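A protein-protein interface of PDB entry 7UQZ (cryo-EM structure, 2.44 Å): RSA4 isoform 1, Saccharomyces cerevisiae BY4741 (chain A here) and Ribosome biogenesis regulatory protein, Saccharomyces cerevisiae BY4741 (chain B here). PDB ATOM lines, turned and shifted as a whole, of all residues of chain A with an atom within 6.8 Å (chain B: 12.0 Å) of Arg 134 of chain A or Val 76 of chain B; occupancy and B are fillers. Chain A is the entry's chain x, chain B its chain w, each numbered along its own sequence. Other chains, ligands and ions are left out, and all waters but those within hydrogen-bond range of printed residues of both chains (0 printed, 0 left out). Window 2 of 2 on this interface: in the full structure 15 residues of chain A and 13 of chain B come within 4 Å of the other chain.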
ATOM      1  N   PRO A 131     -23.563  27.941  -6.369  1.00  0.00           N
ATOM      2  CA  PRO A 131     -23.343  26.728  -7.162  1.00  0.00           C
ATOM      3  C   PRO A 131     -23.382  25.481  -6.296  1.00  0.00           C
ATOM      4  O   PRO A 131     -22.990  25.492  -5.127  1.00  0.00           O
ATOM      5  CB  PRO A 131     -21.947  26.940  -7.763  1.00  0.00           C
ATOM      6  CG  PRO A 131     -21.683  28.408  -7.639  1.00  0.00           C
ATOM      7  CD  PRO A 131     -22.403  28.846  -6.406  1.00  0.00           C
ATOM      8  N   VAL A 132     -23.870  24.395  -6.886  1.00  0.00           N
ATOM      9  CA  VAL A 132     -23.848  23.098  -6.220  1.00  0.00           C
ATOM     10  C   VAL A 132     -22.450  22.511  -6.346  1.00  0.00           C
ATOM     11  O   VAL A 132     -21.899  22.412  -7.450  1.00  0.00           O
ATOM     12  CB  VAL A 132     -24.917  22.163  -6.810  1.00  0.00           C
ATOM     13  CG1 VAL A 132     -26.275  22.490  -6.224  1.00  0.00           C
ATOM     14  CG2 VAL A 132     -24.962  22.282  -8.324  1.00  0.00           C
ATOM     15  N   THR A 133     -21.858  22.143  -5.210  1.00  0.00           N
ATOM     16  CA  THR A 133     -20.475  21.700  -5.171  1.00  0.00           C
ATOM     17  C   THR A 133     -20.291  20.276  -4.670  1.00  0.00           C
ATOM     18  O   THR A 133     -19.160  19.780  -4.686  1.00  0.00           O
ATOM     19  CB  THR A 133     -19.633  22.642  -4.294  1.00  0.00           C
ATOM     20  OG1 THR A 133     -20.197  22.708  -2.979  1.00  0.00           O
ATOM     21  CG2 THR A 133     -19.596  24.041  -4.891  1.00  0.00           C
ATOM     22  N   ARG A 134     -21.353  19.606  -4.231  1.00  0.00           N
ATOM     23  CA  ARG A 134     -21.232  18.263  -3.683  1.00  0.00           C
ATOM     24  C   ARG A 134     -22.567  17.554  -3.820  1.00  0.00           C
ATOM     25  O   ARG A 134     -23.606  18.184  -4.023  1.00  0.00           O
ATOM     26  CB  ARG A 134     -20.792  18.294  -2.217  1.00  0.00           C
ATOM     27  CG  ARG A 134     -21.680  19.146  -1.332  1.00  0.00           C
ATOM     28  CD  ARG A 134     -21.065  19.344   0.043  1.00  0.00           C
ATOM     29  NE  ARG A 134     -21.850  20.264   0.858  1.00  0.00           N
ATOM     30  CZ  ARG A 134     -22.847  19.895   1.649  1.00  0.00           C
ATOM     31  NH1 ARG A 134     -23.206  18.627   1.763  1.00  0.00           N
ATOM     32  NH2 ARG A 134     -23.501  20.821   2.343  1.00  0.00           N
ATOM     33  N   SER A 135     -22.524  16.231  -3.695  1.00  0.00           N
ATOM     34  CA  SER A 135     -23.722  15.409  -3.784  1.00  0.00           C
ATOM     35  C   SER A 135     -24.347  15.275  -2.403  1.00  0.00           C
ATOM     36  O   SER A 135     -23.683  14.841  -1.455  1.00  0.00           O
ATOM     37  CB  SER A 135     -23.395  14.031  -4.357  1.00  0.00           C
ATOM     38  OG  SER A 135     -24.543  13.203  -4.364  1.00  0.00           O
ATOM     39  N   SER A 136     -25.618  15.661  -2.288  1.00  0.00           N
ATOM     40  CA  SER A 136     -26.335  15.460  -1.036  1.00  0.00           C
ATOM     41  C   SER A 136     -26.502  13.976  -0.745  1.00  0.00           C
ATOM     42  O   SER A 136     -26.197  13.512   0.360  1.00  0.00           O
ATOM     43  CB  SER A 136     -27.697  16.150  -1.087  1.00  0.00           C
ATOM     44  OG  SER A 136     -27.618  17.380  -1.778  1.00  0.00           O
ATOM     45  N   SER A 137     -26.963  13.212  -1.734  1.00  0.00           N
ATOM     46  CA  SER A 137     -27.215  11.794  -1.497  1.00  0.00           C
ATOM     47  C   SER A 137     -27.323  11.036  -2.811  1.00  0.00           C
ATOM     48  O   SER A 137     -27.523  11.620  -3.879  1.00  0.00           O
ATOM     49  CB  SER A 137     -28.488  11.583  -0.670  1.00  0.00           C
ATOM     50  OG  SER A 137     -28.679  10.214  -0.363  1.00  0.00           O
ATOM     51  N   VAL A 480     -17.490  24.035 -11.605  1.00  0.00           N
ATOM     52  CA  VAL A 480     -17.202  22.829 -10.831  1.00  0.00           C
ATOM     53  C   VAL A 480     -17.629  21.598 -11.620  1.00  0.00           C
ATOM     54  O   VAL A 480     -18.705  21.563 -12.227  1.00  0.00           O
ATOM     55  CB  VAL A 480     -17.859  22.891  -9.429  1.00  0.00           C
ATOM     56  CG1 VAL A 480     -19.317  23.275  -9.519  1.00  0.00           C
ATOM     57  CG2 VAL A 480     -17.689  21.576  -8.674  1.00  0.00           C
ATOM     58  N   LEU A 482     -18.594  17.605 -11.427  1.00  0.00           N
ATOM     59  CA  LEU A 482     -19.243  16.722 -10.462  1.00  0.00           C
ATOM     60  C   LEU A 482     -19.257  15.292 -10.983  1.00  0.00           C
ATOM     61  O   LEU A 482     -20.110  14.940 -11.819  1.00  0.00           O
ATOM     62  CB  LEU A 482     -20.664  17.202 -10.177  1.00  0.00           C
ATOM     63  CG  LEU A 482     -20.803  18.642  -9.679  1.00  0.00           C
ATOM     64  CD1 LEU A 482     -22.259  19.071  -9.642  1.00  0.00           C
ATOM     65  CD2 LEU A 482     -20.168  18.794  -8.308  1.00  0.00           C
ATOM     66  N   LEU A 512     -28.827  13.568  -5.618  1.00  0.00           N
ATOM     67  CA  LEU A 512     -29.186  14.910  -5.184  1.00  0.00           C
ATOM     68  C   LEU A 512     -27.918  15.648  -4.790  1.00  0.00           C
ATOM     69  O   LEU A 512     -27.099  15.114  -4.033  1.00  0.00           O
ATOM     70  CB  LEU A 512     -30.172  14.875  -4.015  1.00  0.00           C
ATOM     71  CG  LEU A 512     -31.656  14.889  -4.389  1.00  0.00           C
ATOM     72  CD1 LEU A 512     -32.525  14.927  -3.146  1.00  0.00           C
ATOM     73  CD2 LEU A 512     -31.966  16.072  -5.291  1.00  0.00           C
ATOM     74  N   TRP A 513     -27.772  16.870  -5.307  1.00  0.00           N
ATOM     75  CA  TRP A 513     -26.595  17.708  -5.135  1.00  0.00           C
ATOM     76  C   TRP A 513     -27.008  19.028  -4.501  1.00  0.00           C
ATOM     77  O   TRP A 513     -28.027  19.615  -4.881  1.00  0.00           O
ATOM     78  CB  TRP A 513     -25.905  17.994  -6.480  1.00  0.00           C
ATOM     79  CG  TRP A 513     -25.658  16.786  -7.328  1.00  0.00           C
ATOM     80  CD1 TRP A 513     -26.577  16.101  -8.069  1.00  0.00           C
ATOM     81  CD2 TRP A 513     -24.405  16.128  -7.540  1.00  0.00           C
ATOM     82  NE1 TRP A 513     -25.976  15.055  -8.718  1.00  0.00           N
ATOM     83  CE2 TRP A 513     -24.643  15.048  -8.410  1.00  0.00           C
ATOM     84  CE3 TRP A 513     -23.104  16.348  -7.078  1.00  0.00           C
ATOM     85  CZ2 TRP A 513     -23.631  14.187  -8.822  1.00  0.00           C
ATOM     86  CZ3 TRP A 513     -22.104  15.489  -7.482  1.00  0.00           C
ATOM     87  CH2 TRP A 513     -22.370  14.424  -8.350  1.00  0.00           C
ATOM     88  N   THR A 514     -26.200  19.502  -3.554  1.00  0.00           N
ATOM     89  CA  THR A 514     -26.448  20.755  -2.857  1.00  0.00           C
ATOM     90  C   THR A 514     -25.166  21.577  -2.815  1.00  0.00           C
ATOM     91  O   THR A 514     -24.090  21.114  -3.198  1.00  0.00           O
ATOM     92  CB  THR A 514     -26.961  20.518  -1.429  1.00  0.00           C
ATOM     93  OG1 THR A 514     -27.375  21.762  -0.854  1.00  0.00           O
ATOM     94  CG2 THR A 514     -25.864  19.908  -0.569  1.00  0.00           C
ATOM     95  N   HIS A 515     -25.296  22.811  -2.339  1.00  0.00           N
ATOM     96  CA  HIS A 515     -24.152  23.701  -2.178  1.00  0.00           C
ATOM     97  C   HIS A 515     -23.217  23.206  -1.081  1.00  0.00           C
ATOM     98  O   HIS A 515     -21.996  23.316  -1.195  1.00  0.00           O
ATOM     99  CB  HIS A 515     -24.615  25.123  -1.860  1.00  0.00           C
ATOM    100  CG  HIS A 515     -23.510  26.030  -1.417  1.00  0.00           C
ATOM    101  ND1 HIS A 515     -22.559  26.524  -2.282  1.00  0.00           N
ATOM    102  CD2 HIS A 515     -23.199  26.525  -0.195  1.00  0.00           C
ATOM    103  CE1 HIS A 515     -21.713  27.288  -1.615  1.00  0.00           C
ATOM    104  NE2 HIS A 515     -22.079  27.306  -0.347  1.00  0.00           N
ATOM    105  N   THR B  72      -9.386  26.007  -8.513  1.00  0.00           N
ATOM    106  CA  THR B  72      -9.588  24.681  -9.076  1.00  0.00           C
ATOM    107  C   THR B  72     -11.072  24.471  -9.338  1.00  0.00           C
ATOM    108  O   THR B  72     -11.916  25.279  -8.944  1.00  0.00           O
ATOM    109  CB  THR B  72      -9.047  23.585  -8.150  1.00  0.00           C
ATOM    110  OG1 THR B  72      -9.039  22.332  -8.842  1.00  0.00           O
ATOM    111  CG2 THR B  72      -9.915  23.460  -6.910  1.00  0.00           C
ATOM    112  N   THR B  73     -11.384  23.371 -10.020  1.00  0.00           N
ATOM    113  CA  THR B  73     -12.760  22.998 -10.298  1.00  0.00           C
ATOM    114  C   THR B  73     -13.196  21.707  -9.625  1.00  0.00           C
ATOM    115  O   THR B  73     -14.379  21.360  -9.714  1.00  0.00           O
ATOM    116  CB  THR B  73     -12.988  22.862 -11.813  1.00  0.00           C
ATOM    117  OG1 THR B  73     -12.105  21.866 -12.344  1.00  0.00           O
ATOM    118  CG2 THR B  73     -12.735  24.182 -12.515  1.00  0.00           C
ATOM    119  N   GLU B  74     -12.293  20.988  -8.962  1.00  0.00           N
ATOM    120  CA  GLU B  74     -12.665  19.723  -8.347  1.00  0.00           C
ATOM    121  C   GLU B  74     -13.525  19.955  -7.110  1.00  0.00           C
ATOM    122  O   GLU B  74     -13.433  20.988  -6.441  1.00  0.00           O
ATOM    123  CB  GLU B  74     -11.422  18.908  -7.979  1.00  0.00           C
ATOM    124  CG  GLU B  74     -10.613  19.456  -6.816  1.00  0.00           C
ATOM    125  CD  GLU B  74      -9.725  18.401  -6.179  1.00  0.00           C
ATOM    126  OE1 GLU B  74      -9.888  17.207  -6.508  1.00  0.00           O
ATOM    127  OE2 GLU B  74      -8.865  18.762  -5.348  1.00  0.00           O
ATOM    128  N   SER B  75     -14.377  18.977  -6.817  1.00  0.00           N
ATOM    129  CA  SER B  75     -15.321  19.069  -5.718  1.00  0.00           C
ATOM    130  C   SER B  75     -14.688  18.564  -4.423  1.00  0.00           C
ATOM    131  O   SER B  75     -13.530  18.144  -4.384  1.00  0.00           O
ATOM    132  CB  SER B  75     -16.588  18.284  -6.046  1.00  0.00           C
ATOM    133  OG  SER B  75     -17.050  18.591  -7.348  1.00  0.00           O
ATOM    134  N   VAL B  76     -15.469  18.603  -3.346  1.00  0.00           N
ATOM    135  CA  VAL B  76     -15.026  18.117  -2.044  1.00  0.00           C
ATOM    136  C   VAL B  76     -15.086  16.597  -2.030  1.00  0.00           C
ATOM    137  O   VAL B  76     -15.703  15.979  -2.904  1.00  0.00           O
ATOM    138  CB  VAL B  76     -15.877  18.711  -0.908  1.00  0.00           C
ATOM    139  CG1 VAL B  76     -15.734  20.220  -0.870  1.00  0.00           C
ATOM    140  CG2 VAL B  76     -17.329  18.317  -1.084  1.00  0.00           C
ATOM    141  N   GLY B  77     -14.442  15.985  -1.039  1.00  0.00           N
ATOM    142  CA  GLY B  77     -14.383  14.544  -0.936  1.00  0.00           C
ATOM    143  C   GLY B  77     -13.321  13.889  -1.788  1.00  0.00           C
ATOM    144  O   GLY B  77     -13.154  12.665  -1.706  1.00  0.00           O
ATOM    145  N   GLY B  78     -12.597  14.657  -2.599  1.00  0.00           N
ATOM    146  CA  GLY B  78     -11.530  14.123  -3.412  1.00  0.00           C
ATOM    147  C   GLY B  78     -10.168  14.368  -2.786  1.00  0.00           C
ATOM    148  O   GLY B  78     -10.015  15.110  -1.819  1.00  0.00           O
ATOM    149  N   THR B  79      -9.166  13.710  -3.357  1.00  0.00           N
ATOM    150  CA  THR B  79      -7.798  13.906  -2.904  1.00  0.00           C
ATOM    151  C   THR B  79      -7.284  15.267  -3.358  1.00  0.00           C
ATOM    152  O   THR B  79      -7.617  15.741  -4.448  1.00  0.00           O
ATOM    153  CB  THR B  79      -6.899  12.794  -3.441  1.00  0.00           C
ATOM    154  OG1 THR B  79      -6.761  12.932  -4.860  1.00  0.00           O
ATOM    155  CG2 THR B  79      -7.506  11.430  -3.133  1.00  0.00           C
ATOM    156  N   GLY B  80      -6.472  15.899  -2.514  1.00  0.00           N
ATOM    157  CA  GLY B  80      -5.871  17.172  -2.867  1.00  0.00           C
ATOM    158  C   GLY B  80      -6.010  18.245  -1.806  1.00  0.00           C
ATOM    159  O   GLY B  80      -5.084  19.033  -1.590  1.00  0.00           O
ATOM    160  N   GLY B  81      -7.161  18.290  -1.138  1.00  0.00           N
ATOM    161  CA  GLY B  81      -7.380  19.223  -0.056  1.00  0.00           C
ATOM    162  C   GLY B  81      -7.901  20.588  -0.455  1.00  0.00           C
ATOM    163  O   GLY B  81      -8.156  21.415   0.430  1.00  0.00           O
ATOM    164  N   GLN B  82      -8.065  20.861  -1.748  1.00  0.00           N
ATOM    165  CA  GLN B  82      -8.573  22.142  -2.219  1.00  0.00           C
ATOM    166  C   GLN B  82      -9.888  21.935  -2.956  1.00  0.00           C
ATOM    167  O   GLN B  82      -9.979  21.081  -3.845  1.00  0.00           O
ATOM    168  CB  GLN B  82      -7.565  22.839  -3.136  1.00  0.00           C
ATOM    169  CG  GLN B  82      -8.043  24.187  -3.651  1.00  0.00           C
ATOM    170  CD  GLN B  82      -7.049  24.845  -4.582  1.00  0.00           C
ATOM    171  OE1 GLN B  82      -5.988  24.290  -4.867  1.00  0.00           O
ATOM    172  NE2 GLN B  82      -7.384  26.037  -5.060  1.00  0.00           N
ATOM    173  N   SER B  83     -10.897  22.717  -2.589  1.00  0.00           N
ATOM    174  CA  SER B  83     -12.202  22.674  -3.230  1.00  0.00           C
ATOM    175  C   SER B  83     -12.336  23.814  -4.234  1.00  0.00           C
ATOM    176  O   SER B  83     -11.520  24.734  -4.285  1.00  0.00           O
ATOM    177  CB  SER B  83     -13.319  22.745  -2.186  1.00  0.00           C
ATOM    178  OG  SER B  83     -13.315  23.992  -1.514  1.00  0.00           O
ATOM    179  N   SER B  84     -13.399  23.737  -5.039  1.00  0.00           N
ATOM    180  CA  SER B  84     -13.593  24.700  -6.119  1.00  0.00           C
ATOM    181  C   SER B  84     -13.846  26.104  -5.582  1.00  0.00           C
ATOM    182  O   SER B  84     -13.385  27.090  -6.169  1.00  0.00           O
ATOM    183  CB  SER B  84     -14.748  24.255  -7.014  1.00  0.00           C
ATOM    184  OG  SER B  84     -14.894  25.124  -8.122  1.00  0.00           O
ATOM    185  N   VAL B  85     -14.579  26.215  -4.472  1.00  0.00           N
ATOM    186  CA  VAL B  85     -14.860  27.522  -3.894  1.00  0.00           C
ATOM    187  C   VAL B  85     -13.632  28.124  -3.225  1.00  0.00           C
ATOM    188  O   VAL B  85     -13.555  29.348  -3.069  1.00  0.00           O
ATOM    189  CB  VAL B  85     -16.031  27.426  -2.899  1.00  0.00           C
ATOM    190  CG1 VAL B  85     -17.333  27.160  -3.641  1.00  0.00           C
ATOM    191  CG2 VAL B  85     -15.767  26.332  -1.878  1.00  0.00           C
ATOM    192  N   MET B  86     -12.667  27.298  -2.826  1.00  0.00           N
ATOM    193  CA  MET B  86     -11.454  27.790  -2.187  1.00  0.00           C
ATOM    194  C   MET B  86     -10.513  28.398  -3.220  1.00  0.00           C
ATOM    195  O   MET B  86     -10.200  27.769  -4.236  1.00  0.00           O
ATOM    196  CB  MET B  86     -10.746  26.659  -1.444  1.00  0.00           C
ATOM    197  CG  MET B  86     -11.391  26.259  -0.133  1.00  0.00           C
ATOM    198  SD  MET B  86     -10.659  24.753   0.533  1.00  0.00           S
ATOM    199  CE  MET B  86      -8.924  25.196   0.530  1.00  0.00           C
ATOM    200  N   THR B  87     -10.061  29.620  -2.954  1.00  0.00           N
ATOM    201  CA  THR B  87      -9.038  30.284  -3.751  1.00  0.00           C
ATOM    202  C   THR B  87      -7.808  30.463  -2.874  1.00  0.00           C
ATOM    203  O   THR B  87      -7.884  31.106  -1.822  1.00  0.00           O
ATOM    204  CB  THR B  87      -9.532  31.635  -4.273  1.00  0.00           C
ATOM    205  OG1 THR B  87     -10.637  31.432  -5.161  1.00  0.00           O
ATOM    206  CG2 THR B  87      -8.422  32.362  -5.011  1.00  0.00           C
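The backbone carbonyl oxygen (O) of Thr 72 of chain B is in hydrogen-bond range of the side-chain hydroxyl (OG) of Ser 84 of chain B, 3.1 Å away. The backbone carbonyl oxygen of Glu 74 of chain B sits at hydrogen-bond distance from the backbone NH of Ser 84 of chain B (3.1 Å). The backbone carbonyl oxygen (O) of Thr 514 of chain A lies within hydrogen-bond range of the backbone NH (N) of Thr 133 of chain A. The backbone carbonyl oxygen (O) of His 515 of chain A is in hydrogen-bond range of the side-chain hydroxyl (OG1) of Thr 133 of chain A, 2.6 Å away. O of Arg 134 of chain A lies within hydrogen-bond range of N of Thr 514 of chain A.
Thr 133 of chain A touches Ser 75 of chain B. Arg 134 of chain A touches Val 76 of chain B. Val 480 of chain A touches Thr 73 of chain B. Val 480 of chain A touches Ser 75 of chain B (CG2 to OG, 3.3 Å). Val 480 of chain A touches Ser 84 of chain B (CB to OG, 3.9 Å). CD2 of Leu 482 of chain A touches OG of Ser 75 of chain B, at 3.3 Å.
No residue of chain B comes within 4 Å of Val 132 of chain A. Of the printed residues of chain B, Arg 134 of chain A touches Val 76. No residue of chain B comes within 4 Å of Ser 135 of chain A. Of the printed residues of chain A, Ser 75 of chain B touches Thr 133, Val 480 and Leu 482. Val 76 of chain B touches just one residue of chain A: Arg 134 (3.6 Å). Of the printed residues of chain A, Ser 84 of chain B touches Val 480 (3.9 Å). The nearest printed residue of chain A that does not touch Thr 73 of chain B is Leu 482 of chain A (5.9 Å).
Of the 16 printed residues of chain B, 4 touch a printed residue of chain A. Of the 13 printed residues of chain A, 4 touch a printed residue of chain B. Hydrophobic or aromatic side chains of chain A that line the printed part of chain B: Val 480 and Leu 482. Among the printed residues, 6 pairs touch across the chains.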
